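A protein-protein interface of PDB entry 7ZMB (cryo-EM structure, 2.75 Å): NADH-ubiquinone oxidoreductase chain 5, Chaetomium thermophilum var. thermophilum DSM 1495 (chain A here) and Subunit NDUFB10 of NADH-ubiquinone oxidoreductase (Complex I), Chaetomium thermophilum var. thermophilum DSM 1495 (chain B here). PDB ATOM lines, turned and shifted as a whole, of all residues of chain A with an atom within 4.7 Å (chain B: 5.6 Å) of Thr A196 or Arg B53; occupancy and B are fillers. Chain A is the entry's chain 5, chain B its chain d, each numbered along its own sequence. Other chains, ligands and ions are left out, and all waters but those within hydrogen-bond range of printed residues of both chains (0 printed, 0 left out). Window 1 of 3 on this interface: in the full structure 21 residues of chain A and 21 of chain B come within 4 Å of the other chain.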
ATOM      1  N   TRP A  69     -14.297 -10.434  31.780  1.00  0.00           N
ATOM      2  CA  TRP A  69     -15.362 -10.350  30.746  1.00  0.00           C
ATOM      3  C   TRP A  69     -15.877  -8.935  30.579  1.00  0.00           C
ATOM      4  O   TRP A  69     -16.736  -8.729  29.711  1.00  0.00           O
ATOM      5  CB  TRP A  69     -16.549 -11.104  31.345  1.00  0.00           C
ATOM      6  CG  TRP A  69     -16.611 -12.574  31.124  1.00  0.00           C
ATOM      7  CD1 TRP A  69     -16.600 -13.541  32.081  1.00  0.00           C
ATOM      8  CD2 TRP A  69     -16.765 -13.242  29.864  1.00  0.00           C
ATOM      9  NE1 TRP A  69     -16.724 -14.768  31.500  1.00  0.00           N
ATOM     10  CE2 TRP A  69     -16.815 -14.621  30.142  1.00  0.00           C
ATOM     11  CE3 TRP A  69     -16.854 -12.813  28.538  1.00  0.00           C
ATOM     12  CZ2 TRP A  69     -16.945 -15.574  29.136  1.00  0.00           C
ATOM     13  CZ3 TRP A  69     -16.981 -13.758  27.549  1.00  0.00           C
ATOM     14  CH2 TRP A  69     -17.027 -15.119  27.844  1.00  0.00           C
ATOM     15  N   ILE A  71     -15.441  -5.279  29.519  1.00  0.00           N
ATOM     16  CA  ILE A  71     -14.670  -4.326  28.732  1.00  0.00           C
ATOM     17  C   ILE A  71     -15.626  -3.214  28.315  1.00  0.00           C
ATOM     18  O   ILE A  71     -16.287  -3.283  27.274  1.00  0.00           O
ATOM     19  CB  ILE A  71     -13.971  -4.972  27.532  1.00  0.00           C
ATOM     20  CG1 ILE A  71     -13.259  -3.904  26.703  1.00  0.00           C
ATOM     21  CG2 ILE A  71     -14.926  -5.861  26.741  1.00  0.00           C
ATOM     22  CD1 ILE A  71     -12.177  -3.182  27.458  1.00  0.00           C
ATOM     23  N   GLY A 190     -22.455 -11.010  30.953  1.00  0.00           N
ATOM     24  CA  GLY A 190     -20.992 -10.849  30.962  1.00  0.00           C
ATOM     25  C   GLY A 190     -20.558  -9.502  30.433  1.00  0.00           C
ATOM     26  O   GLY A 190     -19.357  -9.232  30.455  1.00  0.00           O
ATOM     27  N   ASN A 191     -21.493  -8.714  29.919  1.00  0.00           N
ATOM     28  CA  ASN A 191     -21.167  -7.333  29.472  1.00  0.00           C
ATOM     29  C   ASN A 191     -22.451  -6.516  29.429  1.00  0.00           C
ATOM     30  O   ASN A 191     -23.499  -7.049  29.799  1.00  0.00           O
ATOM     31  CB  ASN A 191     -20.397  -7.269  28.149  1.00  0.00           C
ATOM     32  CG  ASN A 191     -19.297  -6.231  28.152  1.00  0.00           C
ATOM     33  OD1 ASN A 191     -18.440  -6.229  29.032  1.00  0.00           O
ATOM     34  ND2 ASN A 191     -19.307  -5.350  27.168  1.00  0.00           N
ATOM     35  N   LEU A 192     -22.352  -5.282  28.970  1.00  0.00           N
ATOM     36  CA  LEU A 192     -23.495  -4.398  28.805  1.00  0.00           C
ATOM     37  C   LEU A 192     -23.372  -3.475  27.592  1.00  0.00           C
ATOM     38  O   LEU A 192     -24.070  -2.461  27.529  1.00  0.00           O
ATOM     39  CB  LEU A 192     -23.710  -3.654  30.125  1.00  0.00           C
ATOM     40  CG  LEU A 192     -22.603  -2.768  30.680  1.00  0.00           C
ATOM     41  CD1 LEU A 192     -22.583  -1.406  30.088  1.00  0.00           C
ATOM     42  CD2 LEU A 192     -22.761  -2.691  32.187  1.00  0.00           C
ATOM     43  N   ASP A 193     -22.535  -3.816  26.616  1.00  0.00           N
ATOM     44  CA  ASP A 193     -22.601  -3.173  25.310  1.00  0.00           C
ATOM     45  C   ASP A 193     -23.941  -3.463  24.647  1.00  0.00           C
ATOM     46  O   ASP A 193     -24.462  -4.575  24.735  1.00  0.00           O
ATOM     47  CB  ASP A 193     -21.460  -3.656  24.411  1.00  0.00           C
ATOM     48  CG  ASP A 193     -20.109  -3.158  24.865  1.00  0.00           C
ATOM     49  OD1 ASP A 193     -20.049  -2.064  25.464  1.00  0.00           O
ATOM     50  OD2 ASP A 193     -19.100  -3.852  24.611  1.00  0.00           O
ATOM     51  N   TYR A 194     -24.496  -2.453  23.970  1.00  0.00           N
ATOM     52  CA  TYR A 194     -25.861  -2.569  23.464  1.00  0.00           C
ATOM     53  C   TYR A 194     -25.973  -3.672  22.426  1.00  0.00           C
ATOM     54  O   TYR A 194     -26.987  -4.374  22.363  1.00  0.00           O
ATOM     55  CB  TYR A 194     -26.340  -1.241  22.875  1.00  0.00           C
ATOM     56  CG  TYR A 194     -26.631  -0.183  23.908  1.00  0.00           C
ATOM     57  CD1 TYR A 194     -27.113  -0.521  25.155  1.00  0.00           C
ATOM     58  CD2 TYR A 194     -26.435   1.160  23.628  1.00  0.00           C
ATOM     59  CE1 TYR A 194     -27.376   0.443  26.099  1.00  0.00           C
ATOM     60  CE2 TYR A 194     -26.693   2.126  24.566  1.00  0.00           C
ATOM     61  CZ  TYR A 194     -27.167   1.758  25.798  1.00  0.00           C
ATOM     62  OH  TYR A 194     -27.436   2.716  26.743  1.00  0.00           O
ATOM     63  N   ALA A 195     -24.942  -3.839  21.601  1.00  0.00           N
ATOM     64  CA  ALA A 195     -24.967  -4.897  20.604  1.00  0.00           C
ATOM     65  C   ALA A 195     -25.003  -6.273  21.246  1.00  0.00           C
ATOM     66  O   ALA A 195     -25.568  -7.208  20.673  1.00  0.00           O
ATOM     67  CB  ALA A 195     -23.764  -4.773  19.682  1.00  0.00           C
ATOM     68  N   THR A 196     -24.427  -6.414  22.431  1.00  0.00           N
ATOM     69  CA  THR A 196     -24.338  -7.713  23.078  1.00  0.00           C
ATOM     70  C   THR A 196     -25.570  -8.048  23.907  1.00  0.00           C
ATOM     71  O   THR A 196     -25.961  -9.215  23.968  1.00  0.00           O
ATOM     72  CB  THR A 196     -23.094  -7.764  23.959  1.00  0.00           C
ATOM     73  OG1 THR A 196     -23.279  -6.918  25.097  1.00  0.00           O
ATOM     74  CG2 THR A 196     -21.905  -7.252  23.174  1.00  0.00           C
ATOM     75  N   VAL A 197     -26.195  -7.057  24.540  1.00  0.00           N
ATOM     76  CA  VAL A 197     -27.394  -7.322  25.329  1.00  0.00           C
ATOM     77  C   VAL A 197     -28.571  -7.672  24.425  1.00  0.00           C
ATOM     78  O   VAL A 197     -29.384  -8.541  24.752  1.00  0.00           O
ATOM     79  CB  VAL A 197     -27.715  -6.120  26.238  1.00  0.00           C
ATOM     80  CG1 VAL A 197     -26.747  -6.041  27.390  1.00  0.00           C
ATOM     81  CG2 VAL A 197     -27.648  -4.858  25.457  1.00  0.00           C
ATOM     82  N   PHE A 198     -28.678  -7.013  23.275  1.00  0.00           N
ATOM     83  CA  PHE A 198     -29.864  -7.122  22.435  1.00  0.00           C
ATOM     84  C   PHE A 198     -29.816  -8.312  21.497  1.00  0.00           C
ATOM     85  O   PHE A 198     -30.858  -8.908  21.210  1.00  0.00           O
ATOM     86  CB  PHE A 198     -30.047  -5.845  21.617  1.00  0.00           C
ATOM     87  CG  PHE A 198     -30.224  -4.621  22.453  1.00  0.00           C
ATOM     88  CD1 PHE A 198     -30.662  -4.718  23.754  1.00  0.00           C
ATOM     89  CD2 PHE A 198     -29.960  -3.378  21.938  1.00  0.00           C
ATOM     90  CE1 PHE A 198     -30.833  -3.604  24.519  1.00  0.00           C
ATOM     91  CE2 PHE A 198     -30.126  -2.259  22.705  1.00  0.00           C
ATOM     92  CZ  PHE A 198     -30.561  -2.372  23.996  1.00  0.00           C
ATOM     93  N   SER A 199     -28.628  -8.655  21.010  1.00  0.00           N
ATOM     94  CA  SER A 199     -28.479  -9.859  20.207  1.00  0.00           C
ATOM     95  C   SER A 199     -28.823 -11.098  21.017  1.00  0.00           C
ATOM     96  O   SER A 199     -29.444 -12.034  20.504  1.00  0.00           O
ATOM     97  CB  SER A 199     -27.057  -9.939  19.671  1.00  0.00           C
ATOM     98  OG  SER A 199     -26.141  -9.729  20.725  1.00  0.00           O
ATOM     99  N   LEU A 200     -28.425 -11.089  22.288  1.00  0.00           N
ATOM    100  CA  LEU A 200     -28.630 -12.274  23.157  1.00  0.00           C
ATOM    101  C   LEU A 200     -29.976 -12.226  23.883  1.00  0.00           C
ATOM    102  O   LEU A 200     -30.427 -13.300  24.300  1.00  0.00           O
ATOM    103  CB  LEU A 200     -27.470 -12.361  24.151  1.00  0.00           C
ATOM    104  CG  LEU A 200     -26.103 -12.661  23.544  1.00  0.00           C
ATOM    105  CD1 LEU A 200     -24.995 -12.164  24.453  1.00  0.00           C
ATOM    106  CD2 LEU A 200     -25.946 -14.146  23.287  1.00  0.00           C
ATOM    107  N   MET B  48     -11.317 -15.202  24.595  1.00  0.00           N
ATOM    108  CA  MET B  48     -12.037 -15.646  23.408  1.00  0.00           C
ATOM    109  C   MET B  48     -13.434 -15.054  23.373  1.00  0.00           C
ATOM    110  O   MET B  48     -13.915 -14.645  22.311  1.00  0.00           O
ATOM    111  CB  MET B  48     -12.069 -17.171  23.343  1.00  0.00           C
ATOM    112  CG  MET B  48     -10.694 -17.770  23.119  1.00  0.00           C
ATOM    113  SD  MET B  48     -10.580 -19.556  23.107  1.00  0.00           S
ATOM    114  CE  MET B  48     -11.396 -19.977  21.577  1.00  0.00           C
ATOM    115  N   GLY B  49     -14.044 -14.951  24.550  1.00  0.00           N
ATOM    116  CA  GLY B  49     -15.362 -14.304  24.676  1.00  0.00           C
ATOM    117  C   GLY B  49     -15.269 -12.861  24.211  1.00  0.00           C
ATOM    118  O   GLY B  49     -16.197 -12.407  23.526  1.00  0.00           O
ATOM    119  N   ARG B  50     -14.178 -12.170  24.546  1.00  0.00           N
ATOM    120  CA  ARG B  50     -14.022 -10.763  24.209  1.00  0.00           C
ATOM    121  C   ARG B  50     -13.822 -10.532  22.718  1.00  0.00           C
ATOM    122  O   ARG B  50     -14.033  -9.412  22.246  1.00  0.00           O
ATOM    123  CB  ARG B  50     -12.859 -10.162  24.993  1.00  0.00           C
ATOM    124  CG  ARG B  50     -13.282  -9.634  26.344  1.00  0.00           C
ATOM    125  CD  ARG B  50     -12.101  -9.283  27.200  1.00  0.00           C
ATOM    126  NE  ARG B  50     -11.342  -8.182  26.625  1.00  0.00           N
ATOM    127  CZ  ARG B  50     -10.734  -7.248  27.343  1.00  0.00           C
ATOM    128  NH1 ARG B  50     -10.062  -6.278  26.740  1.00  0.00           N
ATOM    129  NH2 ARG B  50     -10.801  -7.282  28.663  1.00  0.00           N
ATOM    130  N   LEU B  51     -13.420 -11.549  21.971  1.00  0.00           N
ATOM    131  CA  LEU B  51     -13.304 -11.390  20.530  1.00  0.00           C
ATOM    132  C   LEU B  51     -14.586 -11.776  19.812  1.00  0.00           C
ATOM    133  O   LEU B  51     -14.929 -11.166  18.796  1.00  0.00           O
ATOM    134  CB  LEU B  51     -12.133 -12.211  19.989  1.00  0.00           C
ATOM    135  CG  LEU B  51     -10.728 -11.613  20.062  1.00  0.00           C
ATOM    136  CD1 LEU B  51     -10.643 -10.364  19.203  1.00  0.00           C
ATOM    137  CD2 LEU B  51     -10.298 -11.320  21.461  1.00  0.00           C
ATOM    138  N   VAL B  52     -15.299 -12.776  20.332  1.00  0.00           N
ATOM    139  CA  VAL B  52     -16.554 -13.258  19.686  1.00  0.00           C
ATOM    140  C   VAL B  52     -17.618 -12.176  19.886  1.00  0.00           C
ATOM    141  O   VAL B  52     -18.530 -12.086  19.053  1.00  0.00           O
ATOM    142  CB  VAL B  52     -17.012 -14.605  20.286  1.00  0.00           C
ATOM    143  CG1 VAL B  52     -18.354 -15.054  19.738  1.00  0.00           C
ATOM    144  CG2 VAL B  52     -15.973 -15.693  20.077  1.00  0.00           C
ATOM    145  N   ARG B  53     -17.444 -11.323  20.900  1.00  0.00           N
ATOM    146  CA  ARG B  53     -18.453 -10.275  21.181  1.00  0.00           C
ATOM    147  C   ARG B  53     -18.122  -9.151  20.221  1.00  0.00           C
ATOM    148  O   ARG B  53     -19.049  -8.588  19.639  1.00  0.00           O
ATOM    149  CB  ARG B  53     -18.374  -9.812  22.634  1.00  0.00           C
ATOM    150  CG  ARG B  53     -19.581 -10.203  23.471  1.00  0.00           C
ATOM    151  CD  ARG B  53     -19.681  -9.475  24.798  1.00  0.00           C
ATOM    152  NE  ARG B  53     -18.564  -9.677  25.708  1.00  0.00           N
ATOM    153  CZ  ARG B  53     -17.597  -8.794  25.919  1.00  0.00           C
ATOM    154  NH1 ARG B  53     -16.628  -9.066  26.776  1.00  0.00           N
ATOM    155  NH2 ARG B  53     -17.605  -7.640  25.276  1.00  0.00           N
ATOM    156  N   GLU B  54     -16.842  -8.843  20.083  1.00  0.00           N
ATOM    157  CA  GLU B  54     -16.399  -7.872  19.093  1.00  0.00           C
ATOM    158  C   GLU B  54     -16.881  -8.267  17.705  1.00  0.00           C
ATOM    159  O   GLU B  54     -17.407  -7.434  16.959  1.00  0.00           O
ATOM    160  CB  GLU B  54     -14.878  -7.739  19.128  1.00  0.00           C
ATOM    161  CG  GLU B  54     -14.367  -6.739  20.148  1.00  0.00           C
ATOM    162  CD  GLU B  54     -13.069  -6.080  19.720  1.00  0.00           C
ATOM    163  OE1 GLU B  54     -12.536  -6.443  18.651  1.00  0.00           O
ATOM    164  OE2 GLU B  54     -12.581  -5.193  20.452  1.00  0.00           O
ATOM    165  N   GLU B  55     -16.732  -9.544  17.351  1.00  0.00           N
ATOM    166  CA  GLU B  55     -17.251 -10.023  16.076  1.00  0.00           C
ATOM    167  C   GLU B  55     -18.769  -9.941  16.031  1.00  0.00           C
ATOM    168  O   GLU B  55     -19.348  -9.532  15.020  1.00  0.00           O
ATOM    169  CB  GLU B  55     -16.786 -11.456  15.835  1.00  0.00           C
ATOM    170  CG  GLU B  55     -15.293 -11.580  15.648  1.00  0.00           C
ATOM    171  CD  GLU B  55     -14.815 -10.909  14.377  1.00  0.00           C
ATOM    172  OE1 GLU B  55     -15.582 -10.886  13.393  1.00  0.00           O
ATOM    173  OE2 GLU B  55     -13.675 -10.401  14.368  1.00  0.00           O
ATOM    174  N   LEU B  56     -19.428 -10.331  17.120  1.00  0.00           N
ATOM    175  CA  LEU B  56     -20.884 -10.273  17.179  1.00  0.00           C
ATOM    176  C   LEU B  56     -21.392  -8.844  17.076  1.00  0.00           C
ATOM    177  O   LEU B  56     -22.352  -8.570  16.350  1.00  0.00           O
ATOM    178  CB  LEU B  56     -21.359 -10.922  18.472  1.00  0.00           C
ATOM    179  CG  LEU B  56     -22.845 -11.058  18.747  1.00  0.00           C
ATOM    180  CD1 LEU B  56     -23.056 -12.322  19.516  1.00  0.00           C
ATOM    181  CD2 LEU B  56     -23.318  -9.871  19.563  1.00  0.00           C
ATOM    182  N   SER B  57     -20.768  -7.919  17.803  1.00  0.00           N
ATOM    183  CA  SER B  57     -21.213  -6.533  17.762  1.00  0.00           C
ATOM    184  C   SER B  57     -21.079  -5.964  16.361  1.00  0.00           C
ATOM    185  O   SER B  57     -21.896  -5.138  15.934  1.00  0.00           O
ATOM    186  CB  SER B  57     -20.417  -5.696  18.757  1.00  0.00           C
ATOM    187  OG  SER B  57     -20.834  -5.947  20.082  1.00  0.00           O
ATOM    188  N   LYS B  58     -20.052  -6.399  15.630  1.00  0.00           N
ATOM    189  CA  LYS B  58     -19.894  -5.971  14.249  1.00  0.00           C
ATOM    190  C   LYS B  58     -21.099  -6.368  13.408  1.00  0.00           C
ATOM    191  O   LYS B  58     -21.634  -5.543  12.660  1.00  0.00           O
ATOM    192  CB  LYS B  58     -18.607  -6.558  13.669  1.00  0.00           C
ATOM    193  CG  LYS B  58     -17.426  -5.604  13.714  1.00  0.00           C
ATOM    194  CD  LYS B  58     -16.230  -6.147  12.949  1.00  0.00           C
ATOM    195  CE  LYS B  58     -15.265  -6.865  13.879  1.00  0.00           C
ATOM    196  NZ  LYS B  58     -13.910  -7.005  13.274  1.00  0.00           N
ATOM    197  N   TYR B  78     -20.552 -17.226  21.613  1.00  0.00           N
ATOM    198  CA  TYR B  78     -20.372 -16.341  22.785  1.00  0.00           C
ATOM    199  C   TYR B  78     -21.053 -16.971  23.992  1.00  0.00           C
ATOM    200  O   TYR B  78     -20.444 -16.990  25.064  1.00  0.00           O
ATOM    201  CB  TYR B  78     -20.951 -14.942  22.586  1.00  0.00           C
ATOM    202  CG  TYR B  78     -20.808 -14.110  23.834  1.00  0.00           C
ATOM    203  CD1 TYR B  78     -19.556 -13.777  24.318  1.00  0.00           C
ATOM    204  CD2 TYR B  78     -21.911 -13.720  24.572  1.00  0.00           C
ATOM    205  CE1 TYR B  78     -19.403 -13.047  25.482  1.00  0.00           C
ATOM    206  CE2 TYR B  78     -21.776 -12.985  25.737  1.00  0.00           C
ATOM    207  CZ  TYR B  78     -20.517 -12.648  26.195  1.00  0.00           C
ATOM    208  OH  TYR B  78     -20.368 -11.922  27.339  1.00  0.00           O
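Of the 13 printed residues of chain A, 8 touch a printed residue of chain B.
Hydrophobic or aromatic side chains of chain A within 4 Å of the printed part of chain B: Trp A69, Ile A71, Ala A195 and Leu A200.
Among the printed residues, no Asp or Glu carboxylate lies within 4 Å of a Lys or Arg side-chain nitrogen of the other chain.
O of Trp A69 sits at hydrogen-bond distance from NH1 of Arg B53 (3.0 Å).
The guanidinium group of Arg B53 lies close to the side-chain amide nitrogen of Asn A191 (3.4 Å).
The side-chain hydroxyl of Ser B57 lies within hydrogen-bond range of the backbone carbonyl oxygen of Arg B53 (3.2 Å).
The side-chain amide oxygen of Asn A191 sits at hydrogen-bond distance from the backbone NH of Ile A71, at 3.2 Å.
The backbone carbonyl oxygen of Asp A193 is in hydrogen-bond range of the side-chain hydroxyl of Thr A196 (2.6 Å).
The side-chain hydroxyl (OG) of Ser A199 lies within hydrogen-bond range of the backbone carbonyl oxygen (O) of Ala A195, at 2.6 Å.
ND2 of Asn A191 is in hydrogen-bond range of OD2 of Asp A193, 3.0 Å away.
OG of Ser A199 is in hydrogen-bond range of O of Thr A196.
Printed residues of chain B within 4 Å of Ile A71: Arg B50 and Arg B53.
Tyr A194 touches none of the printed residues of chain B.
Printed residues of chain B within 4 Å of Ala A195: Leu B56 and Ser B57.
Thr A196 touches just these residues of chain B: Arg B53 (3.5 Å) and Ser B57 (3.5 Å).
Of the printed residues of chain B, Ser A199 touches Leu B56 (3.1 Å).
Met B48 touches none of the printed residues of chain A.
Printed residues of chain A within 4 Å of Arg B50: Ile A71 (3.8 Å).
Of chain A, only Trp A69, Ile A71, Asn A191 and Thr A196 come within 4 Å of Arg B53.
Among the printed residues, pairs that only touch across the chains: Trp A69 with Gly B49, Trp A69 with Tyr B78, Ile A71 with Arg B50, Ile A71 with Arg B53, Gly A190 with Tyr B78, Ala A195 with Leu B56, Ala A195 with Ser B57, Thr A196 with Arg B53, Thr A196 with Ser B57, Ser A199 with Leu B56 and Leu A200 with Tyr B78.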
